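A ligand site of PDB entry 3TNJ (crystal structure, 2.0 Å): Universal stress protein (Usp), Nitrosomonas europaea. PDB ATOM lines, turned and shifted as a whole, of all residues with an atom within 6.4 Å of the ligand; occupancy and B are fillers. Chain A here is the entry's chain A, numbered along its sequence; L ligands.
The backbone NH of Ala 12 sits at hydrogen-bond distance from the backbone carbonyl oxygen of Val 114, 3.1 Å away. A ring nitrogen (NE2) of His 118 is in hydrogen-bond range of the side-chain carboxylate (OE1) of Glu 18 (2.5 Å). The backbone carbonyl oxygen (O) of Ser 117 lies within hydrogen-bond range of the backbone NH (N) of Leu 147 (2.8 Å). The backbone NH (N) of Asp 14 lies within hydrogen-bond range of the side-chain carboxylate (OD1) of Asp 19 (3.4 Å). O of Ile 40 is in hydrogen-bond range of N of Val 13 (2.9 Å). The backbone NH (N) of Ile 40 lies within hydrogen-bond range of the backbone carbonyl oxygen (O) of Leu 11. The backbone NH (N) of Ser 16 sits at hydrogen-bond distance from the side-chain carboxylate (OD1) of Asp 14 (2.8 Å). A ring nitrogen (ND1) of His 41 is in hydrogen-bond range of the backbone carbonyl oxygen (O) of Val 13, 2.6 Å away.
A ring nitrogen (ND1) of His 118 lies close to an oxygen (O3) of the ligand, at 3.4 Å. The backbone NH (N) of Gly 116 is in hydrogen-bond range of an oxygen (O7) of the ligand (3.0 Å). N3 of the ligand lies within hydrogen-bond range of O of Val 42 (2.7 Å). A nitrogen (N4) of the ligand lies within hydrogen-bond range of the backbone NH of Val 42 (2.9 Å). O2 of the ligand lies within hydrogen-bond range of N of Thr 130 (3.1 Å). The side-chain hydroxyl of Thr 130 lies within hydrogen-bond range of an oxygen (O1) of the ligand, at 2.8 Å. The backbone carbonyl oxygen of Ala 12 is in hydrogen-bond range of an oxygen (O7) of the ligand, 2.8 Å away. The side-chain carboxylate of Asp 44 is in hydrogen-bond range of a nitrogen (N3) of the ligand (3.4 Å).
N4 of the ligand sits close to O of Val 13 (3.3 Å). Residues that only touch the ligand: Asp 14, Ile 40, His 41, Pro 97, Ile 101, Val 115, Ser 129 and Leu 147. 15 residues have an atom within 4 Å of the ligand: Ala 12, Val 13, Asp 14, Ile 40, His 41, Val 42, Asp 44, Pro 97, Ile 101, Val 115, Gly 116, His 118, Ser 129, Thr 130 and Leu 147. Along chain A the residues within 4 Å of the ligand span positions 12 to 147.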
ATOM      1  N   LEU A  11       6.675  -3.802 -17.265  1.00  0.00           N
ATOM      2  CA  LEU A  11       7.095  -4.054 -15.884  1.00  0.00           C
ATOM      3  C   LEU A  11       7.699  -5.471 -15.755  1.00  0.00           C
ATOM      4  O   LEU A  11       7.032  -6.481 -16.043  1.00  0.00           O
ATOM      5  CB  LEU A  11       5.934  -3.897 -14.912  1.00  0.00           C
ATOM      6  CG  LEU A  11       6.293  -4.268 -13.425  1.00  0.00           C
ATOM      7  CD1 LEU A  11       7.406  -3.409 -12.808  1.00  0.00           C
ATOM      8  CD2 LEU A  11       5.052  -4.318 -12.562  1.00  0.00           C
ATOM      9  N   ALA A  12       8.941  -5.508 -15.261  1.00  0.00           N
ATOM     10  CA  ALA A  12       9.695  -6.738 -15.038  1.00  0.00           C
ATOM     11  C   ALA A  12       9.629  -7.098 -13.555  1.00  0.00           C
ATOM     12  O   ALA A  12      10.040  -6.302 -12.696  1.00  0.00           O
ATOM     13  CB  ALA A  12      11.154  -6.562 -15.505  1.00  0.00           C
ATOM     14  N   VAL A  13       9.077  -8.255 -13.231  1.00  0.00           N
ATOM     15  CA  VAL A  13       8.913  -8.665 -11.815  1.00  0.00           C
ATOM     16  C   VAL A  13       9.633  -9.990 -11.564  1.00  0.00           C
ATOM     17  O   VAL A  13       9.521 -10.924 -12.388  1.00  0.00           O
ATOM     18  CB  VAL A  13       7.419  -8.778 -11.376  1.00  0.00           C
ATOM     19  CG1 VAL A  13       6.788  -7.401 -11.089  1.00  0.00           C
ATOM     20  CG2 VAL A  13       6.617  -9.527 -12.409  1.00  0.00           C
ATOM     21  N   ASP A  14      10.382 -10.057 -10.459  1.00  0.00           N
ATOM     22  CA  ASP A  14      11.194 -11.245 -10.097  1.00  0.00           C
ATOM     23  C   ASP A  14      10.535 -12.089  -9.036  1.00  0.00           C
ATOM     24  O   ASP A  14      11.093 -13.103  -8.622  1.00  0.00           O
ATOM     25  CB  ASP A  14      12.616 -10.873  -9.621  1.00  0.00           C
ATOM     26  CG  ASP A  14      12.644 -10.077  -8.334  1.00  0.00           C
ATOM     27  OD1 ASP A  14      11.576  -9.917  -7.690  1.00  0.00           O
ATOM     28  OD2 ASP A  14      13.723  -9.595  -7.927  1.00  0.00           O
ATOM     29  N   PHE A  15       9.354 -11.643  -8.591  1.00  0.00           N
ATOM     30  CA  PHE A  15       8.476 -12.351  -7.641  1.00  0.00           C
ATOM     31  C   PHE A  15       9.027 -12.341  -6.206  1.00  0.00           C
ATOM     32  O   PHE A  15       8.636 -13.151  -5.378  1.00  0.00           O
ATOM     33  CB  PHE A  15       8.136 -13.789  -8.086  1.00  0.00           C
ATOM     34  CG  PHE A  15       7.314 -13.869  -9.361  1.00  0.00           C
ATOM     35  CD1 PHE A  15       6.517 -12.825  -9.808  1.00  0.00           C
ATOM     36  CD2 PHE A  15       7.311 -15.056 -10.074  1.00  0.00           C
ATOM     37  CE1 PHE A  15       5.760 -12.969 -10.978  1.00  0.00           C
ATOM     38  CE2 PHE A  15       6.559 -15.190 -11.227  1.00  0.00           C
ATOM     39  CZ  PHE A  15       5.768 -14.153 -11.660  1.00  0.00           C
ATOM     40  N   SER A  16       9.905 -11.400  -5.925  1.00  0.00           N
ATOM     41  CA  SER A  16      10.421 -11.211  -4.597  1.00  0.00           C
ATOM     42  C   SER A  16       9.397 -10.420  -3.787  1.00  0.00           C
ATOM     43  O   SER A  16       8.382  -9.924  -4.327  1.00  0.00           O
ATOM     44  CB  SER A  16      11.743 -10.437  -4.637  1.00  0.00           C
ATOM     45  OG  SER A  16      11.547  -9.060  -4.931  1.00  0.00           O
ATOM     46  N   GLU A  18      10.016  -7.595  -2.748  1.00  0.00           N
ATOM     47  CA  GLU A  18      10.218  -6.237  -3.296  1.00  0.00           C
ATOM     48  C   GLU A  18       9.225  -5.789  -4.367  1.00  0.00           C
ATOM     49  O   GLU A  18       8.984  -4.592  -4.534  1.00  0.00           O
ATOM     50  CB  GLU A  18      11.640  -6.153  -3.867  1.00  0.00           C
ATOM     51  CG  GLU A  18      12.714  -6.306  -2.785  1.00  0.00           C
ATOM     52  CD  GLU A  18      14.044  -6.862  -3.283  1.00  0.00           C
ATOM     53  OE1 GLU A  18      14.164  -7.261  -4.479  1.00  0.00           O
ATOM     54  OE2 GLU A  18      14.989  -6.914  -2.454  1.00  0.00           O
ATOM     55  N   ASP A  19       8.622  -6.747  -5.065  1.00  0.00           N
ATOM     56  CA  ASP A  19       7.735  -6.432  -6.177  1.00  0.00           C
ATOM     57  C   ASP A  19       6.595  -5.497  -5.754  1.00  0.00           C
ATOM     58  O   ASP A  19       6.200  -4.614  -6.505  1.00  0.00           O
ATOM     59  CB  ASP A  19       7.092  -7.701  -6.745  1.00  0.00           C
ATOM     60  CG  ASP A  19       7.944  -8.409  -7.788  1.00  0.00           C
ATOM     61  OD1 ASP A  19       9.037  -7.925  -8.221  1.00  0.00           O
ATOM     62  OD2 ASP A  19       7.466  -9.495  -8.182  1.00  0.00           O
ATOM     63  N   VAL A  22       6.920  -1.732  -6.452  1.00  0.00           N
ATOM     64  CA  VAL A  22       6.855  -1.360  -7.841  1.00  0.00           C
ATOM     65  C   VAL A  22       5.465  -1.534  -8.462  1.00  0.00           C
ATOM     66  O   VAL A  22       5.120  -0.795  -9.388  1.00  0.00           O
ATOM     67  CB  VAL A  22       7.954  -2.085  -8.636  1.00  0.00           C
ATOM     68  CG1 VAL A  22       7.609  -3.552  -8.804  1.00  0.00           C
ATOM     69  CG2 VAL A  22       8.222  -1.393  -9.968  1.00  0.00           C
ATOM     70  N   ILE A  40       6.322  -8.940 -17.415  1.00  0.00           N
ATOM     71  CA  ILE A  40       7.250 -10.055 -17.698  1.00  0.00           C
ATOM     72  C   ILE A  40       7.882 -10.618 -16.408  1.00  0.00           C
ATOM     73  O   ILE A  40       8.418  -9.886 -15.553  1.00  0.00           O
ATOM     74  CB  ILE A  40       8.362  -9.629 -18.679  1.00  0.00           C
ATOM     75  CG1 ILE A  40       9.238 -10.819 -19.071  1.00  0.00           C
ATOM     76  CG2 ILE A  40       9.222  -8.511 -18.096  1.00  0.00           C
ATOM     77  CD1 ILE A  40      10.202 -10.514 -20.219  1.00  0.00           C
ATOM     78  N   HIS A  41       7.843 -11.950 -16.312  1.00  0.00           N
ATOM     79  CA  HIS A  41       8.731 -12.664 -15.417  1.00  0.00           C
ATOM     80  C   HIS A  41       9.536 -13.687 -16.208  1.00  0.00           C
ATOM     81  O   HIS A  41       9.002 -14.417 -17.078  1.00  0.00           O
ATOM     82  CB  HIS A  41       7.973 -13.307 -14.250  1.00  0.00           C
ATOM     83  CG  HIS A  41       8.852 -14.111 -13.360  1.00  0.00           C
ATOM     84  ND1 HIS A  41       9.637 -13.548 -12.438  1.00  0.00           N
ATOM     85  CD2 HIS A  41       9.110 -15.496 -13.299  1.00  0.00           C
ATOM     86  CE1 HIS A  41      10.351 -14.493 -11.794  1.00  0.00           C
ATOM     87  NE2 HIS A  41      10.025 -15.691 -12.299  1.00  0.00           N
ATOM     88  N   VAL A  42      10.844 -13.698 -15.933  1.00  0.00           N
ATOM     89  CA  VAL A  42      11.788 -14.598 -16.579  1.00  0.00           C
ATOM     90  C   VAL A  42      12.106 -15.774 -15.641  1.00  0.00           C
ATOM     91  O   VAL A  42      12.494 -15.591 -14.469  1.00  0.00           O
ATOM     92  CB  VAL A  42      13.114 -13.900 -17.012  1.00  0.00           C
ATOM     93  CG1 VAL A  42      13.943 -14.873 -17.826  1.00  0.00           C
ATOM     94  CG2 VAL A  42      12.856 -12.629 -17.807  1.00  0.00           C
ATOM     95  N   LEU A  43      11.880 -16.970 -16.146  1.00  0.00           N
ATOM     96  CA  LEU A  43      12.297 -18.194 -15.473  1.00  0.00           C
ATOM     97  C   LEU A  43      13.811 -18.373 -15.654  1.00  0.00           C
ATOM     98  O   LEU A  43      14.293 -18.626 -16.758  1.00  0.00           O
ATOM     99  CB  LEU A  43      11.513 -19.410 -16.029  1.00  0.00           C
ATOM    100  CG  LEU A  43       9.971 -19.344 -15.918  1.00  0.00           C
ATOM    101  CD1 LEU A  43       9.295 -20.336 -16.851  1.00  0.00           C
ATOM    102  CD2 LEU A  43       9.535 -19.580 -14.482  1.00  0.00           C
ATOM    103  N   ASP A  44      14.553 -18.243 -14.554  1.00  0.00           N
ATOM    104  CA  ASP A  44      16.020 -18.410 -14.543  1.00  0.00           C
ATOM    105  C   ASP A  44      16.534 -19.441 -13.521  1.00  0.00           C
ATOM    106  O   ASP A  44      16.595 -20.640 -13.806  1.00  0.00           O
ATOM    107  CB  ASP A  44      16.706 -17.055 -14.293  1.00  0.00           C
ATOM    108  CG  ASP A  44      16.138 -16.315 -13.097  1.00  0.00           C
ATOM    109  OD1 ASP A  44      15.349 -16.917 -12.311  1.00  0.00           O
ATOM    110  OD2 ASP A  44      16.471 -15.111 -12.939  1.00  0.00           O
ATOM    111  N   PRO A  97      17.402 -13.028 -17.463  1.00  0.00           N
ATOM    112  CA  PRO A  97      16.527 -11.879 -17.282  1.00  0.00           C
ATOM    113  C   PRO A  97      16.836 -10.680 -18.175  1.00  0.00           C
ATOM    114  O   PRO A  97      15.958 -10.266 -18.946  1.00  0.00           O
ATOM    115  CB  PRO A  97      16.703 -11.554 -15.791  1.00  0.00           C
ATOM    116  CG  PRO A  97      16.892 -12.896 -15.187  1.00  0.00           C
ATOM    117  CD  PRO A  97      17.713 -13.663 -16.165  1.00  0.00           C
ATOM    118  N   ILE A 101      14.093  -9.723 -21.016  1.00  0.00           N
ATOM    119  CA  ILE A 101      13.415  -8.453 -20.785  1.00  0.00           C
ATOM    120  C   ILE A 101      13.586  -7.534 -21.991  1.00  0.00           C
ATOM    121  O   ILE A 101      12.599  -6.972 -22.493  1.00  0.00           O
ATOM    122  CB  ILE A 101      13.931  -7.729 -19.555  1.00  0.00           C
ATOM    123  CG1 ILE A 101      13.481  -8.433 -18.257  1.00  0.00           C
ATOM    124  CG2 ILE A 101      13.428  -6.296 -19.552  1.00  0.00           C
ATOM    125  CD1 ILE A 101      14.323  -8.008 -17.057  1.00  0.00           C
ATOM    126  N   VAL A 114      10.397  -0.868 -16.885  1.00  0.00           N
ATOM    127  CA  VAL A 114      10.520  -0.636 -15.435  1.00  0.00           C
ATOM    128  C   VAL A 114      11.145  -1.863 -14.749  1.00  0.00           C
ATOM    129  O   VAL A 114      10.657  -2.998 -14.900  1.00  0.00           O
ATOM    130  CB  VAL A 114       9.145  -0.287 -14.831  1.00  0.00           C
ATOM    131  CG1 VAL A 114       9.273   0.009 -13.324  1.00  0.00           C
ATOM    132  CG2 VAL A 114       8.489   0.868 -15.586  1.00  0.00           C
ATOM    133  N   VAL A 115      12.253  -1.622 -14.044  1.00  0.00           N
ATOM    134  CA  VAL A 115      12.959  -2.620 -13.273  1.00  0.00           C
ATOM    135  C   VAL A 115      13.209  -2.094 -11.856  1.00  0.00           C
ATOM    136  O   VAL A 115      13.250  -0.895 -11.629  1.00  0.00           O
ATOM    137  CB  VAL A 115      14.293  -3.018 -13.957  1.00  0.00           C
ATOM    138  CG1 VAL A 115      13.987  -3.749 -15.254  1.00  0.00           C
ATOM    139  CG2 VAL A 115      15.192  -1.801 -14.229  1.00  0.00           C
ATOM    140  N   GLY A 116      13.318  -3.006 -10.894  1.00  0.00           N
ATOM    141  CA  GLY A 116      13.742  -2.683  -9.552  1.00  0.00           C
ATOM    142  C   GLY A 116      15.245  -2.621  -9.469  1.00  0.00           C
ATOM    143  O   GLY A 116      15.941  -3.219 -10.293  1.00  0.00           O
ATOM    144  N   SER A 117      15.741  -1.937  -8.446  1.00  0.00           N
ATOM    145  CA  SER A 117      17.154  -1.755  -8.271  1.00  0.00           C
ATOM    146  C   SER A 117      17.485  -1.712  -6.794  1.00  0.00           C
ATOM    147  O   SER A 117      16.850  -0.992  -6.054  1.00  0.00           O
ATOM    148  CB  SER A 117      17.585  -0.460  -8.918  1.00  0.00           C
ATOM    149  OG  SER A 117      18.980  -0.298  -8.786  1.00  0.00           O
ATOM    150  N   HIS A 118      18.470  -2.499  -6.373  1.00  0.00           N
ATOM    151  CA  HIS A 118      18.930  -2.495  -4.972  1.00  0.00           C
ATOM    152  C   HIS A 118      20.102  -1.569  -4.749  1.00  0.00           C
ATOM    153  O   HIS A 118      20.899  -1.315  -5.653  1.00  0.00           O
ATOM    154  CB  HIS A 118      19.298  -3.895  -4.551  1.00  0.00           C
ATOM    155  CG  HIS A 118      18.197  -4.884  -4.778  1.00  0.00           C
ATOM    156  ND1 HIS A 118      18.272  -5.854  -5.729  1.00  0.00           N
ATOM    157  CD2 HIS A 118      16.963  -5.035  -4.152  1.00  0.00           C
ATOM    158  CE1 HIS A 118      17.137  -6.583  -5.698  1.00  0.00           C
ATOM    159  NE2 HIS A 118      16.343  -6.088  -4.733  1.00  0.00           N
ATOM    160  N   GLY A 128      26.998  -5.682 -12.241  1.00  0.00           N
ATOM    161  CA  GLY A 128      26.379  -6.959 -12.692  1.00  0.00           C
ATOM    162  C   GLY A 128      24.872  -7.141 -12.458  1.00  0.00           C
ATOM    163  O   GLY A 128      24.319  -8.174 -12.830  1.00  0.00           O
ATOM    164  N   SER A 129      24.219  -6.139 -11.854  1.00  0.00           N
ATOM    165  CA  SER A 129      22.762  -6.208 -11.555  1.00  0.00           C
ATOM    166  C   SER A 129      21.870  -6.225 -12.827  1.00  0.00           C
ATOM    167  O   SER A 129      22.289  -5.780 -13.897  1.00  0.00           O
ATOM    168  CB  SER A 129      22.342  -5.053 -10.621  1.00  0.00           C
ATOM    169  OG  SER A 129      22.202  -3.806 -11.311  1.00  0.00           O
ATOM    170  N   THR A 130      20.642  -6.716 -12.689  1.00  0.00           N
ATOM    171  CA  THR A 130      19.711  -6.735 -13.821  1.00  0.00           C
ATOM    172  C   THR A 130      19.400  -5.286 -14.283  1.00  0.00           C
ATOM    173  O   THR A 130      19.471  -4.984 -15.486  1.00  0.00           O
ATOM    174  CB  THR A 130      18.409  -7.512 -13.524  1.00  0.00           C
ATOM    175  OG1 THR A 130      18.720  -8.813 -13.018  1.00  0.00           O
ATOM    176  CG2 THR A 130      17.513  -7.656 -14.792  1.00  0.00           C
ATOM    177  N   ALA A 131      19.090  -4.394 -13.328  1.00  0.00           N
ATOM    178  CA  ALA A 131      18.808  -2.993 -13.686  1.00  0.00           C
ATOM    179  C   ALA A 131      19.931  -2.392 -14.558  1.00  0.00           C
ATOM    180  O   ALA A 131      19.691  -1.868 -15.643  1.00  0.00           O
ATOM    181  CB  ALA A 131      18.642  -2.145 -12.444  1.00  0.00           C
ATOM    182  N   LEU A 147      14.550  -0.118  -4.709  1.00  0.00           N
ATOM    183  CA  LEU A 147      13.841  -1.088  -3.846  1.00  0.00           C
ATOM    184  C   LEU A 147      14.380  -1.008  -2.413  1.00  0.00           C
ATOM    185  O   LEU A 147      15.532  -0.623  -2.190  1.00  0.00           O
ATOM    186  CB  LEU A 147      14.017  -2.512  -4.357  1.00  0.00           C
ATOM    187  CG  LEU A 147      13.511  -2.828  -5.767  1.00  0.00           C
ATOM    188  CD1 LEU A 147      14.109  -4.149  -6.244  1.00  0.00           C
ATOM    189  CD2 LEU A 147      11.997  -2.832  -5.775  1.00  0.00           C
HETATM  190  P1  LIG L   1      18.407  -8.208  -9.460  1.00  0.00           P
HETATM  191  O1  LIG L   1      18.456  -9.487 -10.308  1.00  0.00           O
HETATM  192  O2  LIG L   1      19.351  -7.122  -9.890  1.00  0.00           O
HETATM  193  O3  LIG L   1      18.314  -8.461  -7.974  1.00  0.00           O
HETATM  194  O4  LIG L   1      16.894  -7.720  -9.800  1.00  0.00           O
HETATM  195  C1  LIG L   1      16.254  -6.481  -9.489  1.00  0.00           C
HETATM  196  C2  LIG L   1      15.141  -6.266 -10.527  1.00  0.00           C
HETATM  197  O5  LIG L   1      15.478  -6.844 -11.788  1.00  0.00           O
HETATM  198  C3  LIG L   1      13.780  -6.860 -10.217  1.00  0.00           C
HETATM  199  O6  LIG L   1      12.935  -5.995  -9.455  1.00  0.00           O
HETATM  200  C4  LIG L   1      13.183  -7.035 -11.581  1.00  0.00           C
HETATM  201  O7  LIG L   1      12.735  -5.733 -11.974  1.00  0.00           O
HETATM  202  C5  LIG L   1      14.344  -7.395 -12.448  1.00  0.00           C
HETATM  203  N1  LIG L   1      14.478  -8.864 -12.465  1.00  0.00           N
HETATM  204  C6  LIG L   1      15.447  -9.622 -11.880  1.00  0.00           C
HETATM  205  N2  LIG L   1      15.207 -10.940 -12.099  1.00  0.00           N
HETATM  206  C7  LIG L   1      14.074 -11.026 -12.865  1.00  0.00           C
HETATM  207  C8  LIG L   1      13.259 -12.100 -13.483  1.00  0.00           C
HETATM  208  N3  LIG L   1      13.581 -13.411 -13.327  1.00  0.00           N
HETATM  209  N4  LIG L   1      12.171 -11.731 -14.204  1.00  0.00           N
HETATM  210  C9  LIG L   1      11.823 -10.453 -14.370  1.00  0.00           C
HETATM  211  N5  LIG L   1      12.491  -9.416 -13.815  1.00  0.00           N
HETATM  212  C10 LIG L   1      13.612  -9.647 -13.099  1.00  0.00           C
